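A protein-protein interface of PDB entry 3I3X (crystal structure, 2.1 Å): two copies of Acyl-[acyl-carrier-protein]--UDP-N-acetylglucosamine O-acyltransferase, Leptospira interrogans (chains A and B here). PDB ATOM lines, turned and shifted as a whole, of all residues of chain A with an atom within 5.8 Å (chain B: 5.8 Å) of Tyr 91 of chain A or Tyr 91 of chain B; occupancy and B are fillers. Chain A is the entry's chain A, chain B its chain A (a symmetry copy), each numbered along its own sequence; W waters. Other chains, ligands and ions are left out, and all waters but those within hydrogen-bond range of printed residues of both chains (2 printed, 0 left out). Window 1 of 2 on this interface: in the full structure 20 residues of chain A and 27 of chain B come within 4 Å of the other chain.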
ATOM      1  N   HIS A  42      25.473   6.726  19.292  1.00  0.00           N
ATOM      2  CA  HIS A  42      24.800   8.008  19.015  1.00  0.00           C
ATOM      3  C   HIS A  42      25.724   9.145  18.552  1.00  0.00           C
ATOM      4  O   HIS A  42      25.381  10.316  18.691  1.00  0.00           O
ATOM      5  CB  HIS A  42      23.961   8.462  20.223  1.00  0.00           C
ATOM      6  CG  HIS A  42      23.166   7.364  20.854  1.00  0.00           C
ATOM      7  ND1 HIS A  42      23.512   6.797  22.062  1.00  0.00           N
ATOM      8  CD2 HIS A  42      22.052   6.713  20.438  1.00  0.00           C
ATOM      9  CE1 HIS A  42      22.640   5.852  22.369  1.00  0.00           C
ATOM     10  NE2 HIS A  42      21.744   5.781  21.401  1.00  0.00           N
ATOM     11  N   HIS A  58      33.246   9.650  21.934  1.00  0.00           N
ATOM     12  CA  HIS A  58      32.300   9.136  22.929  1.00  0.00           C
ATOM     13  C   HIS A  58      30.868   9.432  22.573  1.00  0.00           C
ATOM     14  O   HIS A  58      30.593  10.249  21.698  1.00  0.00           O
ATOM     15  CB  HIS A  58      32.603   9.733  24.302  1.00  0.00           C
ATOM     16  CG  HIS A  58      33.786   9.119  24.975  1.00  0.00           C
ATOM     17  ND1 HIS A  58      35.065   9.230  24.477  1.00  0.00           N
ATOM     18  CD2 HIS A  58      33.887   8.396  26.113  1.00  0.00           C
ATOM     19  CE1 HIS A  58      35.901   8.591  25.275  1.00  0.00           C
ATOM     20  NE2 HIS A  58      35.210   8.080  26.279  1.00  0.00           N
ATOM     21  N   GLN A  59      29.956   8.795  23.294  1.00  0.00           N
ATOM     22  CA  GLN A  59      28.529   8.877  23.024  1.00  0.00           C
ATOM     23  C   GLN A  59      27.947  10.277  22.816  1.00  0.00           C
ATOM     24  O   GLN A  59      28.084  11.159  23.673  1.00  0.00           O
ATOM     25  CB  GLN A  59      27.733   8.161  24.118  1.00  0.00           C
ATOM     26  CG  GLN A  59      26.327   8.703  24.224  1.00  0.00           C
ATOM     27  CD  GLN A  59      25.278   7.666  24.522  1.00  0.00           C
ATOM     28  OE1 GLN A  59      25.473   6.468  24.272  1.00  0.00           O
ATOM     29  NE2 GLN A  59      24.127   8.128  25.041  1.00  0.00           N
ATOM     30  N   GLY A  60      27.279  10.462  21.680  1.00  0.00           N
ATOM     31  CA  GLY A  60      26.522  11.681  21.416  1.00  0.00           C
ATOM     32  C   GLY A  60      27.328  12.835  20.834  1.00  0.00           C
ATOM     33  O   GLY A  60      26.765  13.870  20.507  1.00  0.00           O
ATOM     34  N   ALA A  61      28.640  12.652  20.711  1.00  0.00           N
ATOM     35  CA  ALA A  61      29.517  13.626  20.059  1.00  0.00           C
ATOM     36  C   ALA A  61      29.051  13.875  18.639  1.00  0.00           C
ATOM     37  O   ALA A  61      28.630  12.954  17.925  1.00  0.00           O
ATOM     38  CB  ALA A  61      30.968  13.158  20.068  1.00  0.00           C
ATOM     39  N   VAL A  62      29.137  15.129  18.228  1.00  0.00           N
ATOM     40  CA  VAL A  62      28.585  15.557  16.966  1.00  0.00           C
ATOM     41  C   VAL A  62      29.682  16.307  16.221  1.00  0.00           C
ATOM     42  O   VAL A  62      30.210  17.314  16.715  1.00  0.00           O
ATOM     43  CB  VAL A  62      27.289  16.357  17.220  1.00  0.00           C
ATOM     44  CG1 VAL A  62      27.199  17.583  16.373  1.00  0.00           C
ATOM     45  CG2 VAL A  62      26.067  15.460  17.041  1.00  0.00           C
ATOM     46  N   ARG A  89      34.792  13.814  24.004  1.00  0.00           N
ATOM     47  CA  ARG A  89      33.943  13.234  25.045  1.00  0.00           C
ATOM     48  C   ARG A  89      32.455  13.436  24.767  1.00  0.00           C
ATOM     49  O   ARG A  89      32.090  14.070  23.776  1.00  0.00           O
ATOM     50  CB  ARG A  89      34.352  13.744  26.434  1.00  0.00           C
ATOM     51  CG  ARG A  89      35.747  13.263  26.870  1.00  0.00           C
ATOM     52  CD  ARG A  89      35.827  11.728  26.973  1.00  0.00           C
ATOM     53  NE  ARG A  89      34.786  11.185  27.843  1.00  0.00           N
ATOM     54  CZ  ARG A  89      34.992  10.696  29.062  1.00  0.00           C
ATOM     55  NH1 ARG A  89      36.213  10.649  29.558  1.00  0.00           N
ATOM     56  NH2 ARG A  89      33.971  10.239  29.777  1.00  0.00           N
ATOM     57  N   GLU A  90      31.613  12.888  25.647  1.00  0.00           N
ATOM     58  CA  GLU A  90      30.164  12.821  25.432  1.00  0.00           C
ATOM     59  C   GLU A  90      29.555  14.170  25.077  1.00  0.00           C
ATOM     60  O   GLU A  90      29.790  15.163  25.758  1.00  0.00           O
ATOM     61  CB  GLU A  90      29.435  12.207  26.638  1.00  0.00           C
ATOM     62  CG  GLU A  90      29.704  10.703  26.880  1.00  0.00           C
ATOM     63  CD  GLU A  90      31.076  10.391  27.465  1.00  0.00           C
ATOM     64  OE1 GLU A  90      31.834  11.330  27.787  1.00  0.00           O
ATOM     65  OE2 GLU A  90      31.411   9.192  27.604  1.00  0.00           O
ATOM     66  N   TYR A  91      28.799  14.190  23.983  1.00  0.00           N
ATOM     67  CA  TYR A  91      28.074  15.382  23.525  1.00  0.00           C
ATOM     68  C   TYR A  91      28.947  16.604  23.196  1.00  0.00           C
ATOM     69  O   TYR A  91      28.443  17.720  23.103  1.00  0.00           O
ATOM     70  CB  TYR A  91      26.940  15.746  24.498  1.00  0.00           C
ATOM     71  CG  TYR A  91      26.047  14.572  24.779  1.00  0.00           C
ATOM     72  CD1 TYR A  91      26.052  13.949  26.025  1.00  0.00           C
ATOM     73  CD2 TYR A  91      25.226  14.047  23.782  1.00  0.00           C
ATOM     74  CE1 TYR A  91      25.240  12.847  26.279  1.00  0.00           C
ATOM     75  CE2 TYR A  91      24.416  12.945  24.024  1.00  0.00           C
ATOM     76  CZ  TYR A  91      24.435  12.346  25.268  1.00  0.00           C
ATOM     77  OH  TYR A  91      23.628  11.253  25.503  1.00  0.00           O
ATOM     78  N   SER A  92      30.243  16.379  22.997  1.00  0.00           N
ATOM     79  CA  SER A  92      31.123  17.436  22.511  1.00  0.00           C
ATOM     80  C   SER A  92      30.689  17.722  21.085  1.00  0.00           C
ATOM     81  O   SER A  92      30.207  16.832  20.381  1.00  0.00           O
ATOM     82  CB  SER A  92      32.606  17.079  22.657  1.00  0.00           C
ATOM     83  OG  SER A  92      32.960  15.936  21.894  1.00  0.00           O
ATOM     84  N   ASN A  93      30.887  18.965  20.656  1.00  0.00           N
ATOM     85  CA  ASN A  93      30.236  19.489  19.466  1.00  0.00           C
ATOM     86  C   ASN A  93      31.213  20.304  18.609  1.00  0.00           C
ATOM     87  O   ASN A  93      31.643  21.391  19.011  1.00  0.00           O
ATOM     88  CB  ASN A  93      29.025  20.332  19.904  1.00  0.00           C
ATOM     89  CG  ASN A  93      28.124  20.730  18.750  1.00  0.00           C
ATOM     90  OD1 ASN A  93      28.500  20.604  17.577  1.00  0.00           O
ATOM     91  ND2 ASN A  93      26.916  21.214  19.084  1.00  0.00           N
ATOM     92  N   GLY A 114      33.287  16.632  27.881  1.00  0.00           N
ATOM     93  CA  GLY A 114      31.850  16.571  27.593  1.00  0.00           C
ATOM     94  C   GLY A 114      31.265  17.947  27.344  1.00  0.00           C
ATOM     95  O   GLY A 114      31.675  18.925  27.986  1.00  0.00           O
ATOM     96  N   ASN A 115      30.343  18.021  26.415  1.00  0.00           N
ATOM     97  CA  ASN A 115      29.616  19.223  26.109  1.00  0.00           C
ATOM     98  C   ASN A 115      30.457  20.457  25.753  1.00  0.00           C
ATOM     99  O   ASN A 115      29.997  21.517  25.801  1.00  0.00           O
ATOM    100  CB  ASN A 115      28.609  19.562  27.197  1.00  0.00           C
ATOM    101  CG  ASN A 115      27.536  18.561  27.312  1.00  0.00           C
ATOM    102  OD1 ASN A 115      27.672  17.563  27.979  1.00  0.00           O
ATOM    103  ND2 ASN A 115      26.467  18.793  26.646  1.00  0.00           N
ATOM    104  N   SER A 116      31.690  20.272  25.374  1.00  0.00           N
ATOM    105  CA  SER A 116      32.552  21.363  24.960  1.00  0.00           C
ATOM    106  C   SER A 116      32.327  21.606  23.469  1.00  0.00           C
ATOM    107  O   SER A 116      31.902  20.697  22.741  1.00  0.00           O
ATOM    108  CB  SER A 116      34.020  21.075  25.305  1.00  0.00           C
ATOM    109  OG  SER A 116      34.574  20.058  24.477  1.00  0.00           O
ATOM    110  N   HIS B  42      17.759   6.777  24.782  1.00  0.00           N
ATOM    111  CA  HIS B  42      19.161   7.174  24.553  1.00  0.00           C
ATOM    112  C   HIS B  42      20.005   7.353  25.824  1.00  0.00           C
ATOM    113  O   HIS B  42      21.011   8.057  25.804  1.00  0.00           O
ATOM    114  CB  HIS B  42      19.239   8.439  23.680  1.00  0.00           C
ATOM    115  CG  HIS B  42      18.304   8.427  22.513  1.00  0.00           C
ATOM    116  ND1 HIS B  42      17.157   9.191  22.472  1.00  0.00           N
ATOM    117  CD2 HIS B  42      18.333   7.730  21.350  1.00  0.00           C
ATOM    118  CE1 HIS B  42      16.526   8.974  21.330  1.00  0.00           C
ATOM    119  NE2 HIS B  42      17.217   8.092  20.632  1.00  0.00           N
ATOM    120  N   HIS B  58      16.354  10.605  32.484  1.00  0.00           N
ATOM    121  CA  HIS B  58      15.775  11.198  31.276  1.00  0.00           C
ATOM    122  C   HIS B  58      16.656  11.025  30.067  1.00  0.00           C
ATOM    123  O   HIS B  58      17.828  10.675  30.187  1.00  0.00           O
ATOM    124  CB  HIS B  58      15.518  12.689  31.492  1.00  0.00           C
ATOM    125  CG  HIS B  58      14.309  12.974  32.321  1.00  0.00           C
ATOM    126  ND1 HIS B  58      14.215  12.612  33.646  1.00  0.00           N
ATOM    127  CD2 HIS B  58      13.149  13.597  32.018  1.00  0.00           C
ATOM    128  CE1 HIS B  58      13.041  12.989  34.118  1.00  0.00           C
ATOM    129  NE2 HIS B  58      12.377  13.595  33.150  1.00  0.00           N
ATOM    130  N   GLN B  59      16.095  11.321  28.903  1.00  0.00           N
ATOM    131  CA  GLN B  59      16.758  11.115  27.626  1.00  0.00           C
ATOM    132  C   GLN B  59      18.194  11.631  27.504  1.00  0.00           C
ATOM    133  O   GLN B  59      18.467  12.816  27.732  1.00  0.00           O
ATOM    134  CB  GLN B  59      15.919  11.694  26.484  1.00  0.00           C
ATOM    135  CG  GLN B  59      16.775  12.044  25.290  1.00  0.00           C
ATOM    136  CD  GLN B  59      16.130  11.771  23.958  1.00  0.00           C
ATOM    137  OE1 GLN B  59      15.203  10.957  23.850  1.00  0.00           O
ATOM    138  NE2 GLN B  59      16.642  12.441  22.911  1.00  0.00           N
ATOM    139  N   GLY B  60      19.100  10.734  27.121  1.00  0.00           N
ATOM    140  CA  GLY B  60      20.471  11.110  26.793  1.00  0.00           C
ATOM    141  C   GLY B  60      21.424  11.192  27.978  1.00  0.00           C
ATOM    142  O   GLY B  60      22.612  11.423  27.792  1.00  0.00           O
ATOM    143  N   ALA B  61      20.901  11.007  29.186  1.00  0.00           N
ATOM    144  CA  ALA B  61      21.717  10.940  30.400  1.00  0.00           C
ATOM    145  C   ALA B  61      22.743   9.832  30.275  1.00  0.00           C
ATOM    146  O   ALA B  61      22.463   8.748  29.742  1.00  0.00           O
ATOM    147  CB  ALA B  61      20.853  10.727  31.638  1.00  0.00           C
ATOM    148  N   VAL B  62      23.935  10.106  30.779  1.00  0.00           N
ATOM    149  CA  VAL B  62      25.061   9.223  30.594  1.00  0.00           C
ATOM    150  C   VAL B  62      25.666   8.966  31.969  1.00  0.00           C
ATOM    151  O   VAL B  62      26.084   9.904  32.663  1.00  0.00           O
ATOM    152  CB  VAL B  62      26.023   9.832  29.551  1.00  0.00           C
ATOM    153  CG1 VAL B  62      27.455   9.713  29.955  1.00  0.00           C
ATOM    154  CG2 VAL B  62      25.773   9.216  28.177  1.00  0.00           C
ATOM    155  N   ARG B  89      18.280  14.498  34.753  1.00  0.00           N
ATOM    156  CA  ARG B  89      17.594  15.099  33.609  1.00  0.00           C
ATOM    157  C   ARG B  89      18.379  14.947  32.309  1.00  0.00           C
ATOM    158  O   ARG B  89      19.485  14.403  32.311  1.00  0.00           O
ATOM    159  CB  ARG B  89      17.222  16.562  33.898  1.00  0.00           C
ATOM    160  CG  ARG B  89      16.166  16.711  35.005  1.00  0.00           C
ATOM    161  CD  ARG B  89      14.834  16.031  34.633  1.00  0.00           C
ATOM    162  NE  ARG B  89      14.321  16.501  33.348  1.00  0.00           N
ATOM    163  CZ  ARG B  89      13.280  17.312  33.195  1.00  0.00           C
ATOM    164  NH1 ARG B  89      12.607  17.730  34.249  1.00  0.00           N
ATOM    165  NH2 ARG B  89      12.905  17.692  31.979  1.00  0.00           N
ATOM    166  N   GLU B  90      17.793  15.425  31.208  1.00  0.00           N
ATOM    167  CA  GLU B  90      18.316  15.191  29.858  1.00  0.00           C
ATOM    168  C   GLU B  90      19.788  15.554  29.722  1.00  0.00           C
ATOM    169  O   GLU B  90      20.202  16.644  30.103  1.00  0.00           O
ATOM    170  CB  GLU B  90      17.485  15.920  28.789  1.00  0.00           C
ATOM    171  CG  GLU B  90      16.051  15.378  28.580  1.00  0.00           C
ATOM    172  CD  GLU B  90      15.069  15.740  29.688  1.00  0.00           C
ATOM    173  OE1 GLU B  90      15.437  16.497  30.611  1.00  0.00           O
ATOM    174  OE2 GLU B  90      13.912  15.262  29.645  1.00  0.00           O
ATOM    175  N   TYR B  91      20.567  14.611  29.201  1.00  0.00           N
ATOM    176  CA  TYR B  91      21.998  14.805  28.930  1.00  0.00           C
ATOM    177  C   TYR B  91      22.866  15.142  30.153  1.00  0.00           C
ATOM    178  O   TYR B  91      23.988  15.616  30.006  1.00  0.00           O
ATOM    179  CB  TYR B  91      22.210  15.819  27.792  1.00  0.00           C
ATOM    180  CG  TYR B  91      21.410  15.464  26.572  1.00  0.00           C
ATOM    181  CD1 TYR B  91      20.312  16.230  26.188  1.00  0.00           C
ATOM    182  CD2 TYR B  91      21.720  14.331  25.822  1.00  0.00           C
ATOM    183  CE1 TYR B  91      19.556  15.890  25.069  1.00  0.00           C
ATOM    184  CE2 TYR B  91      20.970  13.980  24.707  1.00  0.00           C
ATOM    185  CZ  TYR B  91      19.887  14.756  24.343  1.00  0.00           C
ATOM    186  OH  TYR B  91      19.147  14.403  23.234  1.00  0.00           O
ATOM    187  N   SER B  92      22.349  14.869  31.349  1.00  0.00           N
ATOM    188  CA  SER B  92      23.154  14.987  32.559  1.00  0.00           C
ATOM    189  C   SER B  92      24.203  13.893  32.476  1.00  0.00           C
ATOM    190  O   SER B  92      23.963  12.833  31.892  1.00  0.00           O
ATOM    191  CB  SER B  92      22.305  14.950  33.835  1.00  0.00           C
ATOM    192  OG  SER B  92      21.613  13.719  33.981  1.00  0.00           O
ATOM    193  N   ASN B  93      25.357  14.147  33.085  1.00  0.00           N
ATOM    194  CA  ASN B  93      26.560  13.374  32.823  1.00  0.00           C
ATOM    195  C   ASN B  93      27.310  13.050  34.121  1.00  0.00           C
ATOM    196  O   ASN B  93      27.870  13.948  34.762  1.00  0.00           O
ATOM    197  CB  ASN B  93      27.442  14.165  31.838  1.00  0.00           C
ATOM    198  CG  ASN B  93      28.608  13.357  31.299  1.00  0.00           C
ATOM    199  OD1 ASN B  93      28.934  12.282  31.821  1.00  0.00           O
ATOM    200  ND2 ASN B  93      29.243  13.877  30.236  1.00  0.00           N
ATOM    201  N   GLY B 114      19.256  19.251  33.451  1.00  0.00           N
ATOM    202  CA  GLY B 114      19.815  18.957  32.126  1.00  0.00           C
ATOM    203  C   GLY B 114      21.249  19.426  32.001  1.00  0.00           C
ATOM    204  O   GLY B 114      21.614  20.477  32.551  1.00  0.00           O
ATOM    205  N   ASN B 115      22.051  18.651  31.311  1.00  0.00           N
ATOM    206  CA  ASN B 115      23.419  18.982  31.015  1.00  0.00           C
ATOM    207  C   ASN B 115      24.320  19.301  32.216  1.00  0.00           C
ATOM    208  O   ASN B 115      25.317  19.869  32.070  1.00  0.00           O
ATOM    209  CB  ASN B 115      23.515  20.084  29.971  1.00  0.00           C
ATOM    210  CG  ASN B 115      22.993  19.671  28.658  1.00  0.00           C
ATOM    211  OD1 ASN B 115      21.817  19.749  28.392  1.00  0.00           O
ATOM    212  ND2 ASN B 115      23.849  19.200  27.827  1.00  0.00           N
ATOM    213  N   SER B 116      23.941  18.893  33.393  1.00  0.00           N
ATOM    214  CA  SER B 116      24.746  19.090  34.584  1.00  0.00           C
ATOM    215  C   SER B 116      25.721  17.919  34.698  1.00  0.00           C
ATOM    216  O   SER B 116      25.460  16.829  34.168  1.00  0.00           O
ATOM    217  CB  SER B 116      23.865  19.258  35.831  1.00  0.00           C
ATOM    218  OG  SER B 116      23.241  18.036  36.212  1.00  0.00           O
HETATM  219  O   HOH W   1      27.180  17.944  30.768  1.00  0.00           O
HETATM  220  O   HOH W   2      31.601  13.595  29.426  1.00  0.00           O
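The backbone carbonyl oxygen (O) of His 42 of chain B lies within hydrogen-bond range of the side-chain amide nitrogen (NE2) of Gln 59 of chain A (3.2 Å).
The side-chain hydroxyl (OH) of Tyr 91 of chain A is in hydrogen-bond range of the backbone carbonyl oxygen (O) of Gly 60 of chain B (2.5 Å).
The side-chain amide nitrogen (ND2) of Asn 115 of chain A lies close to the side-chain amide nitrogen (ND2) of Asn 115 of chain B, at 2.9 Å.
ND1 of His 42 of chain B sits at hydrogen-bond distance from OE1 of Gln 59 of chain B (3.0 Å).
The backbone carbonyl oxygen (O) of Gln 59 of chain A is in hydrogen-bond range of the backbone NH (N) of Tyr 91 of chain A (3.1 Å).
O of Glu 90 of chain B is in hydrogen-bond range of N of Asn 115 of chain B, at 3.0 Å.
The guanidinium group of Arg 89 of chain A is in salt-bridge range of the side-chain carboxylate of Glu 90 of chain A (3.0 Å).
N of Asn 115 of chain A is in hydrogen-bond range of O of Glu 90 of chain A, 3.0 Å away.
O of Ser 92 of chain B lies within hydrogen-bond range of N of Val 62 of chain B (2.9 Å).
NE2 of His 42 of chain A touches CD2 of His 42 of chain B, at 3.9 Å.
NE2 of Gln 59 of chain A touches CG2 of Val 62 of chain B, 3.7 Å away.
Glu 90 of chain A touches Val 62 of chain B.
CB of Glu 90 of chain A touches ND2 of Asn 93 of chain B (3.97 Å).
Tyr 91 of chain A touches Val 62 of chain B.
Tyr 91 of chain A touches Tyr 91 of chain B (CZ to CD2, 3.4 Å).
Gln 59 of chain B touches none of the printed residues of chain A.
Of the printed residues of chain A, Gly 60 of chain B touches Tyr 91.
Printed residues of chain A within 4 Å of Val 62 of chain B: Gln 59, Glu 90 and Tyr 91.
Tyr 91 of chain B touches just one residue of chain A: Tyr 91.
Printed residues of chain A within 4 Å of Asn 93 of chain B: Glu 90 (3.97 Å).
The nearest residue of chain A that does not touch Tyr 91 of chain B is Asn 115 of chain A (4.6 Å).
The nearest printed residue of chain A that does not touch His 42 of chain B is Tyr 91 of chain A (4.1 Å).
Of the 14 printed residues of chain A, 5 touch a printed residue of chain B.
Printed residues of chain A that touch a printed residue of chain B: His 42, Gln 59, Glu 90, Tyr 91 and Asn 115.
Among the printed residues, 9 pairs touch across the chains.
Glu 90 of chain A touches Val 62 of chain B, but with the chains exchanged Val 62 of chain A does not touch Glu 90 of chain B (14.2 Å).
Glu 90 of chain A touches Asn 93 of chain B, but with the chains exchanged Asn 93 of chain A does not touch Glu 90 of chain B (13.7 Å).
Tyr 91 of chain A touches Gly 60 of chain B, but with the chains exchanged Gly 60 of chain A does not touch Tyr 91 of chain B (6.9 Å).
Tyr 91 of chain A touches Val 62 of chain B, but with the chains exchanged Val 62 of chain A does not touch Tyr 91 of chain B (9.3 Å).
Positions printed for both chains: 42, 58, 59, 60, 61, 62, 89, 90, 91, 92, 93, 114, 115 and 116.
Of the 9 pairs that touch across the chains among the printed residues, 3 have their exchanged pair printed and touching as well.
Water W2 bridges ND2 of Asn 93 of chain B (2.5 Å) and OE1 of Glu 90 of chain A (2.8 Å).
Water W1 bridges OD1 of Asn 115 of chain A (2.9 Å) and O of Asn 115 of chain B (3.0 Å).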
